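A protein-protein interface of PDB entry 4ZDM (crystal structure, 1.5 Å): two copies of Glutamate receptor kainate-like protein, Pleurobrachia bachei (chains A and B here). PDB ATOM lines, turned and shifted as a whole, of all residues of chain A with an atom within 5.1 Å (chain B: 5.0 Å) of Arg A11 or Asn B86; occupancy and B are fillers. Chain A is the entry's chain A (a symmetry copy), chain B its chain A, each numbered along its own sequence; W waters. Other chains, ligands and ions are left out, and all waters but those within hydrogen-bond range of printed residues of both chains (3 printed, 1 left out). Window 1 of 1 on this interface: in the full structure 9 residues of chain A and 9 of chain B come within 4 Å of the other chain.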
ATOM      1  N   MET A   8       3.604 -10.385  14.299  1.00  0.00           N
ATOM      2  CA  MET A   8       3.693 -10.676  12.866  1.00  0.00           C
ATOM      3  C   MET A   8       2.595  -9.959  12.123  1.00  0.00           C
ATOM      4  O   MET A   8       1.484  -9.862  12.608  1.00  0.00           O
ATOM      5  CB  MET A   8       3.547 -12.203  12.615  1.00  0.00           C
ATOM      6  CG  MET A   8       3.797 -12.674  11.209  1.00  0.00           C
ATOM      7  SD  MET A   8       3.569 -14.495  11.163  1.00  0.00           S
ATOM      8  CE  MET A   8       4.165 -14.770   9.489  1.00  0.00           C
ATOM      9  N   HIS A   9       2.890  -9.545  10.901  1.00  0.00           N
ATOM     10  CA  HIS A   9       1.909  -8.957  10.002  1.00  0.00           C
ATOM     11  C   HIS A   9       1.466  -9.966   8.964  1.00  0.00           C
ATOM     12  O   HIS A   9       2.351 -10.505   8.252  1.00  0.00           O
ATOM     13  CB  HIS A   9       2.531  -7.757   9.301  1.00  0.00           C
ATOM     14  CG  HIS A   9       1.542  -7.018   8.499  1.00  0.00           C
ATOM     15  ND1 HIS A   9       0.534  -6.281   9.076  1.00  0.00           N
ATOM     16  CD2 HIS A   9       1.364  -6.926   7.157  1.00  0.00           C
ATOM     17  CE1 HIS A   9      -0.261  -5.801   8.127  1.00  0.00           C
ATOM     18  NE2 HIS A   9       0.255  -6.144   6.952  1.00  0.00           N
ATOM     19  N   LEU A  10       0.173 -10.173   8.841  1.00  0.00           N
ATOM     20  CA  LEU A  10      -0.415 -11.064   7.840  1.00  0.00           C
ATOM     21  C   LEU A  10      -1.293 -10.353   6.867  1.00  0.00           C
ATOM     22  O   LEU A  10      -2.006  -9.410   7.238  1.00  0.00           O
ATOM     23  CB  LEU A  10      -1.227 -12.164   8.519  1.00  0.00           C
ATOM     24  CG  LEU A  10      -0.526 -13.035   9.543  1.00  0.00           C
ATOM     25  CD1 LEU A  10      -1.563 -14.019  10.155  1.00  0.00           C
ATOM     26  CD2 LEU A  10       0.635 -13.788   8.947  1.00  0.00           C
ATOM     27  N   ARG A  11      -1.259 -10.761   5.610  1.00  0.00           N
ATOM     28  CA  ARG A  11      -2.211 -10.319   4.610  1.00  0.00           C
ATOM     29  C   ARG A  11      -3.216 -11.454   4.450  1.00  0.00           C
ATOM     30  O   ARG A  11      -2.870 -12.614   4.287  1.00  0.00           O
ATOM     31  CB  ARG A  11      -1.571  -9.997   3.279  1.00  0.00           C
ATOM     32  CG  ARG A  11      -0.858  -8.667   3.231  1.00  0.00           C
ATOM     33  CD  ARG A  11       0.574  -8.779   3.709  1.00  0.00           C
ATOM     34  NE  ARG A  11       1.270  -7.497   3.493  1.00  0.00           N
ATOM     35  CZ  ARG A  11       2.551  -7.296   3.720  1.00  0.00           C
ATOM     36  NH1 ARG A  11       3.326  -8.270   4.138  1.00  0.00           N
ATOM     37  NH2 ARG A  11       3.045  -6.092   3.519  1.00  0.00           N
ATOM     38  N   LEU A  12      -4.495 -11.115   4.538  1.00  0.00           N
ATOM     39  CA  LEU A  12      -5.570 -12.095   4.573  1.00  0.00           C
ATOM     40  C   LEU A  12      -6.447 -11.927   3.345  1.00  0.00           C
ATOM     41  O   LEU A  12      -6.950 -10.841   3.049  1.00  0.00           O
ATOM     42  CB  LEU A  12      -6.385 -11.965   5.857  1.00  0.00           C
ATOM     43  CG  LEU A  12      -5.570 -12.097   7.129  1.00  0.00           C
ATOM     44  CD1 LEU A  12      -6.478 -11.915   8.325  1.00  0.00           C
ATOM     45  CD2 LEU A  12      -4.789 -13.355   7.279  1.00  0.00           C
ATOM     46  N   GLY A  13      -6.683 -13.038   2.650  1.00  0.00           N
ATOM     47  CA  GLY A  13      -7.436 -13.021   1.425  1.00  0.00           C
ATOM     48  C   GLY A  13      -8.938 -13.066   1.658  1.00  0.00           C
ATOM     49  O   GLY A  13      -9.430 -13.911   2.398  1.00  0.00           O
ATOM     50  N   ASN A  57      -4.119  -6.896   7.220  1.00  0.00           N
ATOM     51  CA  ASN A  57      -4.990  -6.234   6.287  1.00  0.00           C
ATOM     52  C   ASN A  57      -5.601  -7.244   5.360  1.00  0.00           C
ATOM     53  O   ASN A  57      -5.167  -8.431   5.341  1.00  0.00           O
ATOM     54  CB  ASN A  57      -4.264  -5.158   5.481  1.00  0.00           C
ATOM     55  CG  ASN A  57      -3.934  -3.963   6.347  1.00  0.00           C
ATOM     56  OD1 ASN A  57      -4.821  -3.331   6.909  1.00  0.00           O
ATOM     57  ND2 ASN A  57      -2.643  -3.718   6.577  1.00  0.00           N
ATOM     58  N   ILE A  59      -6.837  -8.475   1.425  1.00  0.00           N
ATOM     59  CA  ILE A  59      -6.525  -8.304   0.025  1.00  0.00           C
ATOM     60  C   ILE A  59      -7.549  -9.096  -0.749  1.00  0.00           C
ATOM     61  O   ILE A  59      -7.762 -10.296  -0.498  1.00  0.00           O
ATOM     62  CB  ILE A  59      -5.096  -8.777  -0.350  1.00  0.00           C
ATOM     63  CG1 ILE A  59      -4.054  -7.849   0.335  1.00  0.00           C
ATOM     64  CG2 ILE A  59      -4.931  -8.824  -1.891  1.00  0.00           C
ATOM     65  CD1 ILE A  59      -2.641  -8.121  -0.060  1.00  0.00           C
ATOM     66  N   LYS A  87       1.107 -13.334  -2.076  1.00  0.00           N
ATOM     67  CA  LYS A  87       0.445 -12.047  -1.967  1.00  0.00           C
ATOM     68  C   LYS A  87      -0.341 -11.975  -0.655  1.00  0.00           C
ATOM     69  O   LYS A  87      -0.361 -10.942   0.029  1.00  0.00           O
ATOM     70  CB  LYS A  87      -0.447 -11.825  -3.190  1.00  0.00           C
ATOM     71  CG  LYS A  87      -1.066 -10.436  -3.202  1.00  0.00           C
ATOM     72  CD  LYS A  87      -1.499  -9.985  -4.566  1.00  0.00           C
ATOM     73  CE  LYS A  87      -1.888  -8.484  -4.533  1.00  0.00           C
ATOM     74  NZ  LYS A  87      -0.747  -7.635  -4.116  1.00  0.00           N
ATOM     75  N   THR A  88      -0.996 -13.078  -0.312  1.00  0.00           N
ATOM     76  CA  THR A  88      -1.607 -13.249   0.992  1.00  0.00           C
ATOM     77  C   THR A  88      -0.962 -14.376   1.743  1.00  0.00           C
ATOM     78  O   THR A  88      -0.219 -15.174   1.177  1.00  0.00           O
ATOM     79  CB  THR A  88      -3.101 -13.526   0.878  1.00  0.00           C
ATOM     80  OG1 THR A  88      -3.255 -14.658   0.005  1.00  0.00           O
ATOM     81  CG2 THR A  88      -3.841 -12.317   0.318  1.00  0.00           C
ATOM     82  N   ASP A  89      -1.205 -14.416   3.046  1.00  0.00           N
ATOM     83  CA  ASP A  89      -0.686 -15.452   3.947  1.00  0.00           C
ATOM     84  C   ASP A  89      -1.732 -16.434   4.455  1.00  0.00           C
ATOM     85  O   ASP A  89      -1.385 -17.546   4.900  1.00  0.00           O
ATOM     86  CB  ASP A  89      -0.026 -14.777   5.139  1.00  0.00           C
ATOM     87  CG  ASP A  89       1.043 -13.830   4.713  1.00  0.00           C
ATOM     88  OD1 ASP A  89       2.039 -14.275   4.066  1.00  0.00           O
ATOM     89  OD2 ASP A  89       0.917 -12.604   4.946  1.00  0.00           O
ATOM     90  N   MET A  90      -3.018 -16.068   4.391  1.00  0.00           N
ATOM     91  CA  MET A  90      -4.086 -16.944   4.803  1.00  0.00           C
ATOM     92  C   MET A  90      -5.357 -16.476   4.136  1.00  0.00           C
ATOM     93  O   MET A  90      -5.554 -15.263   4.006  1.00  0.00           O
ATOM     94  CB  MET A  90      -4.221 -16.972   6.356  1.00  0.00           C
ATOM     95  CG  MET A  90      -5.289 -17.888   6.850  1.00  0.00           C
ATOM     96  SD  MET A  90      -5.152 -18.285   8.629  1.00  0.00           S
ATOM     97  CE  MET A  90      -5.384 -16.710   9.335  1.00  0.00           C
ATOM     98  N   ARG B  11       7.497  -8.068  -0.876  1.00  0.00           N
ATOM     99  CA  ARG B  11       7.487  -6.693  -0.418  1.00  0.00           C
ATOM    100  C   ARG B  11       8.922  -6.370  -0.015  1.00  0.00           C
ATOM    101  O   ARG B  11       9.575  -7.101   0.712  1.00  0.00           O
ATOM    102  CB  ARG B  11       6.553  -6.458   0.747  1.00  0.00           C
ATOM    103  CG  ARG B  11       5.092  -6.374   0.373  1.00  0.00           C
ATOM    104  CD  ARG B  11       4.442  -7.741   0.336  1.00  0.00           C
ATOM    105  NE  ARG B  11       2.991  -7.593   0.126  1.00  0.00           N
ATOM    106  CZ  ARG B  11       2.130  -8.589   0.135  1.00  0.00           C
ATOM    107  NH1 ARG B  11       2.520  -9.819   0.376  1.00  0.00           N
ATOM    108  NH2 ARG B  11       0.861  -8.328  -0.101  1.00  0.00           N
ATOM    109  N   ARG B  32       4.312   2.995  -2.737  1.00  0.00           N
ATOM    110  CA  ARG B  32       4.816   1.623  -2.867  1.00  0.00           C
ATOM    111  C   ARG B  32       5.215   1.260  -4.275  1.00  0.00           C
ATOM    112  O   ARG B  32       5.816   0.226  -4.513  1.00  0.00           O
ATOM    113  CB  ARG B  32       3.777   0.609  -2.387  1.00  0.00           C
ATOM    114  CG  ARG B  32       3.426   0.744  -0.917  1.00  0.00           C
ATOM    115  CD  ARG B  32       2.727  -0.521  -0.456  1.00  0.00           C
ATOM    116  NE  ARG B  32       2.447  -0.519   0.961  1.00  0.00           N
ATOM    117  CZ  ARG B  32       1.905  -1.540   1.621  1.00  0.00           C
ATOM    118  NH1 ARG B  32       1.550  -2.643   0.987  1.00  0.00           N
ATOM    119  NH2 ARG B  32       1.749  -1.418   2.930  1.00  0.00           N
ATOM    120  N   ILE B  59       8.065  -0.878   0.481  1.00  0.00           N
ATOM    121  CA  ILE B  59       7.425  -0.430   1.696  1.00  0.00           C
ATOM    122  C   ILE B  59       8.464   0.333   2.478  1.00  0.00           C
ATOM    123  O   ILE B  59       9.575  -0.165   2.734  1.00  0.00           O
ATOM    124  CB  ILE B  59       6.859  -1.589   2.557  1.00  0.00           C
ATOM    125  CG1 ILE B  59       5.684  -2.264   1.798  1.00  0.00           C
ATOM    126  CG2 ILE B  59       6.442  -1.066   3.956  1.00  0.00           C
ATOM    127  CD1 ILE B  59       4.966  -3.309   2.586  1.00  0.00           C
ATOM    128  N   ASP B  82      10.425  -4.145  10.247  1.00  0.00           N
ATOM    129  CA  ASP B  82       9.432  -4.501   9.239  1.00  0.00           C
ATOM    130  C   ASP B  82       9.737  -5.877   8.657  1.00  0.00           C
ATOM    131  O   ASP B  82       8.834  -6.670   8.353  1.00  0.00           O
ATOM    132  CB  ASP B  82       9.370  -3.464   8.107  1.00  0.00           C
ATOM    133  CG  ASP B  82       8.480  -2.279   8.424  1.00  0.00           C
ATOM    134  OD1 ASP B  82       7.975  -2.159   9.584  1.00  0.00           O
ATOM    135  OD2 ASP B  82       8.356  -1.404   7.493  1.00  0.00           O
ATOM    136  N   LEU B  83      11.003  -6.191   8.421  1.00  0.00           N
ATOM    137  CA  LEU B  83      11.425  -7.503   7.916  1.00  0.00           C
ATOM    138  C   LEU B  83      11.120  -8.624   8.923  1.00  0.00           C
ATOM    139  O   LEU B  83      10.536  -9.650   8.572  1.00  0.00           O
ATOM    140  CB  LEU B  83      12.913  -7.463   7.579  1.00  0.00           C
ATOM    141  CG  LEU B  83      13.523  -8.760   7.092  1.00  0.00           C
ATOM    142  CD1 LEU B  83      12.991  -9.168   5.722  1.00  0.00           C
ATOM    143  CD2 LEU B  83      15.023  -8.657   7.043  1.00  0.00           C
ATOM    144  N   LEU B  84      11.504  -8.419  10.176  1.00  0.00           N
ATOM    145  CA  LEU B  84      11.216  -9.438  11.194  1.00  0.00           C
ATOM    146  C   LEU B  84       9.744  -9.666  11.417  1.00  0.00           C
ATOM    147  O   LEU B  84       9.332 -10.806  11.697  1.00  0.00           O
ATOM    148  CB  LEU B  84      11.907  -9.055  12.495  1.00  0.00           C
ATOM    149  CG  LEU B  84      13.411  -9.187  12.478  1.00  0.00           C
ATOM    150  CD1 LEU B  84      14.066  -8.532  13.697  1.00  0.00           C
ATOM    151  CD2 LEU B  84      13.860 -10.625  12.367  1.00  0.00           C
ATOM    152  N   ASP B  85       8.954  -8.628  11.240  1.00  0.00           N
ATOM    153  CA  ASP B  85       7.513  -8.734  11.400  1.00  0.00           C
ATOM    154  C   ASP B  85       6.811  -9.294  10.174  1.00  0.00           C
ATOM    155  O   ASP B  85       5.593  -9.400  10.173  1.00  0.00           O
ATOM    156  CB  ASP B  85       6.894  -7.359  11.686  1.00  0.00           C
ATOM    157  CG  ASP B  85       7.203  -6.821  13.064  1.00  0.00           C
ATOM    158  OD1 ASP B  85       7.608  -7.604  13.935  1.00  0.00           O
ATOM    159  OD2 ASP B  85       6.972  -5.583  13.244  1.00  0.00           O
ATOM    160  N   ASN B  86       7.530  -9.579   9.081  1.00  0.00           N
ATOM    161  CA  ASN B  86       6.931 -10.060   7.851  1.00  0.00           C
ATOM    162  C   ASN B  86       6.126  -8.993   7.124  1.00  0.00           C
ATOM    163  O   ASN B  86       5.424  -9.320   6.154  1.00  0.00           O
ATOM    164  CB  ASN B  86       6.049 -11.300   8.115  1.00  0.00           C
ATOM    165  CG  ASN B  86       6.293 -12.401   7.129  1.00  0.00           C
ATOM    166  OD1 ASN B  86       5.772 -12.402   6.062  1.00  0.00           O
ATOM    167  ND2 ASN B  86       7.071 -13.381   7.518  1.00  0.00           N
ATOM    168  N   LYS B  87       6.312  -7.730   7.477  1.00  0.00           N
ATOM    169  CA  LYS B  87       5.734  -6.673   6.669  1.00  0.00           C
ATOM    170  C   LYS B  87       6.447  -6.604   5.315  1.00  0.00           C
ATOM    171  O   LYS B  87       5.817  -6.411   4.264  1.00  0.00           O
ATOM    172  CB  LYS B  87       5.809  -5.347   7.430  1.00  0.00           C
ATOM    173  CG  LYS B  87       5.099  -4.223   6.691  1.00  0.00           C
ATOM    174  CD  LYS B  87       4.692  -3.085   7.581  1.00  0.00           C
ATOM    175  CE  LYS B  87       3.770  -2.107   6.808  1.00  0.00           C
ATOM    176  NZ  LYS B  87       2.535  -2.778   6.338  1.00  0.00           N
ATOM    177  N   THR B  88       7.764  -6.757   5.347  1.00  0.00           N
ATOM    178  CA  THR B  88       8.559  -6.933   4.146  1.00  0.00           C
ATOM    179  C   THR B  88       9.222  -8.279   4.134  1.00  0.00           C
ATOM    180  O   THR B  88       9.268  -8.974   5.145  1.00  0.00           O
ATOM    181  CB  THR B  88       9.631  -5.857   4.022  1.00  0.00           C
ATOM    182  OG1 THR B  88      10.395  -5.879   5.240  1.00  0.00           O
ATOM    183  CG2 THR B  88       9.005  -4.483   3.811  1.00  0.00           C
ATOM    184  N   ASP B  89       9.697  -8.678   2.962  1.00  0.00           N
ATOM    185  CA  ASP B  89      10.398  -9.949   2.750  1.00  0.00           C
ATOM    186  C   ASP B  89      11.893  -9.816   2.495  1.00  0.00           C
ATOM    187  O   ASP B  89      12.649 -10.792   2.674  1.00  0.00           O
ATOM    188  CB  ASP B  89       9.761 -10.669   1.570  1.00  0.00           C
ATOM    189  CG  ASP B  89       8.299 -10.871   1.775  1.00  0.00           C
ATOM    190  OD1 ASP B  89       7.903 -11.564   2.761  1.00  0.00           O
ATOM    191  OD2 ASP B  89       7.480 -10.310   1.008  1.00  0.00           O
ATOM    192  N   ARG B 222      15.197 -12.492   6.168  1.00  0.00           N
ATOM    193  CA  ARG B 222      15.005 -13.310   7.366  1.00  0.00           C
ATOM    194  C   ARG B 222      15.905 -14.533   7.293  1.00  0.00           C
ATOM    195  O   ARG B 222      16.220 -15.042   6.225  1.00  0.00           O
ATOM    196  CB  ARG B 222      13.523 -13.729   7.528  1.00  0.00           C
ATOM    197  CG  ARG B 222      12.618 -12.593   7.934  1.00  0.00           C
ATOM    198  CD  ARG B 222      11.185 -13.081   8.133  1.00  0.00           C
ATOM    199  NE  ARG B 222      10.552 -13.492   6.893  1.00  0.00           N
ATOM    200  CZ  ARG B 222       9.987 -12.629   6.045  1.00  0.00           C
ATOM    201  NH1 ARG B 222       9.950 -11.350   6.319  1.00  0.00           N
ATOM    202  NH2 ARG B 222       9.461 -13.073   4.901  1.00  0.00           N
HETATM  203  O   HOH W   1       3.187 -12.240   2.514  1.00  0.00           O
HETATM  204  O   HOH W   2       5.294 -10.834   3.488  1.00  0.00           O
HETATM  205  O   HOH W   3       4.447 -14.636   5.133  1.00  0.00           O
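The backbone carbonyl oxygen of Lys A87 lies within hydrogen-bond range of the guanidinium group of Arg B11 (2.9 Å). O of Asp B85 is in hydrogen-bond range of N of His A9, at 2.8 Å. O of Asn B86 lies within hydrogen-bond range of NH1 of Arg A11. The backbone carbonyl oxygen (O) of Lys B87 is in hydrogen-bond range of the guanidinium group (NH2) of Arg A11, at 2.9 Å.
O of Arg B11 sits at hydrogen-bond distance from N of Asp B89. The backbone NH (N) of Lys B87 is in hydrogen-bond range of the backbone carbonyl oxygen (O) of Asp B82 (2.9 Å). The backbone carbonyl oxygen of Arg A11 lies within hydrogen-bond range of the backbone NH of Asp A89 (2.7 Å). The backbone carbonyl oxygen of Arg A11 is in hydrogen-bond range of the backbone NH of Met A90. The backbone carbonyl oxygen of Leu A12 lies within hydrogen-bond range of the backbone NH of Ile A59 (2.9 Å).
Met A8 touches Asp B85. CE of Met A8 touches ND2 of Asn B86 (3.8 Å). CB of Asn B86 touches O of His A9, 3.8 Å away. Arg B11 touches Arg A11 (NE to CZ, 3.6 Å). Arg A11 touches Ile B59 (NH2 to CD1, 3.5 Å). Ile A59 touches Arg B11 (CD1 to NH2, 3.5 Å).
Of the printed residues of chain B, Met A8 touches Asp B85 and Asn B86. Printed residues of chain B within 4 Å of His A9: Asp B85 (2.8 Å) and Asn B86 (3.8 Å). Of chain B, only Arg B11 (3.6 Å), Ile B59 (3.5 Å), Asn B86 (3.1 Å) and Lys B87 (2.9 Å) come within 4 Å of Arg A11. Of the printed residues of chain A, Arg B11 touches Arg A11 (3.6 Å), Ile A59 (3.5 Å) and Lys A87 (2.9 Å). Printed residues of chain A within 4 Å of Asp B85: Met A8 (3.5 Å) and His A9 (2.8 Å). Of chain A, only Met A8 (3.8 Å), His A9 (3.8 Å) and Arg A11 (3.1 Å) come within 4 Å of Asn B86. Of the printed residues of chain A, Lys B87 touches Arg A11. The nearest residue of chain B that does not touch Arg A11 is Arg B32 (4.5 Å).
Of the 12 printed residues of chain A, 5 touch a printed residue of chain B. Hydrophobic or aromatic side chains of chain A within 4 Å of the printed part of chain B: Met A8, His A9 and Ile A59. Along chain A the printed residues that touch a printed residue of chain B span positions 8 to 87. Of the 12 printed residues of chain B, 5 touch a printed residue of chain A. Printed residues of chain B that touch a printed residue of chain A: Arg B11, Ile B59, Asp B85, Asn B86 and Lys B87. Hydrophobic or aromatic side chains of chain B within 4 Å of the printed part of chain A: Ile B59.
Arg A11 touches its own counterpart, Arg B11. Arg A11 touches Ile B59, and with the chains exchanged Ile A59 touches Arg B11. Arg A11 touches Lys B87, and with the chains exchanged Lys A87 touches Arg B11. Of the 10 pairs that touch across the chains among the printed residues, 5 have their exchanged pair printed and touching as well.
Water W3 lies within hydrogen-bond range of OD1 of Asp A89 and OD1 of Asn B86. Water W2 lies within hydrogen-bond range of the side-chain carboxylate (OD1) of Asp B89 (2.8 Å), the side-chain amide oxygen (OD1) of Asn B86 (3.1 Å) and the guanidinium group (NH1) of Arg A11 (3.3 Å). Water W1 lies within hydrogen-bond range of OD1 of Asp A89 (2.8 Å) and NH1 of Arg B11 (3.3 Å).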
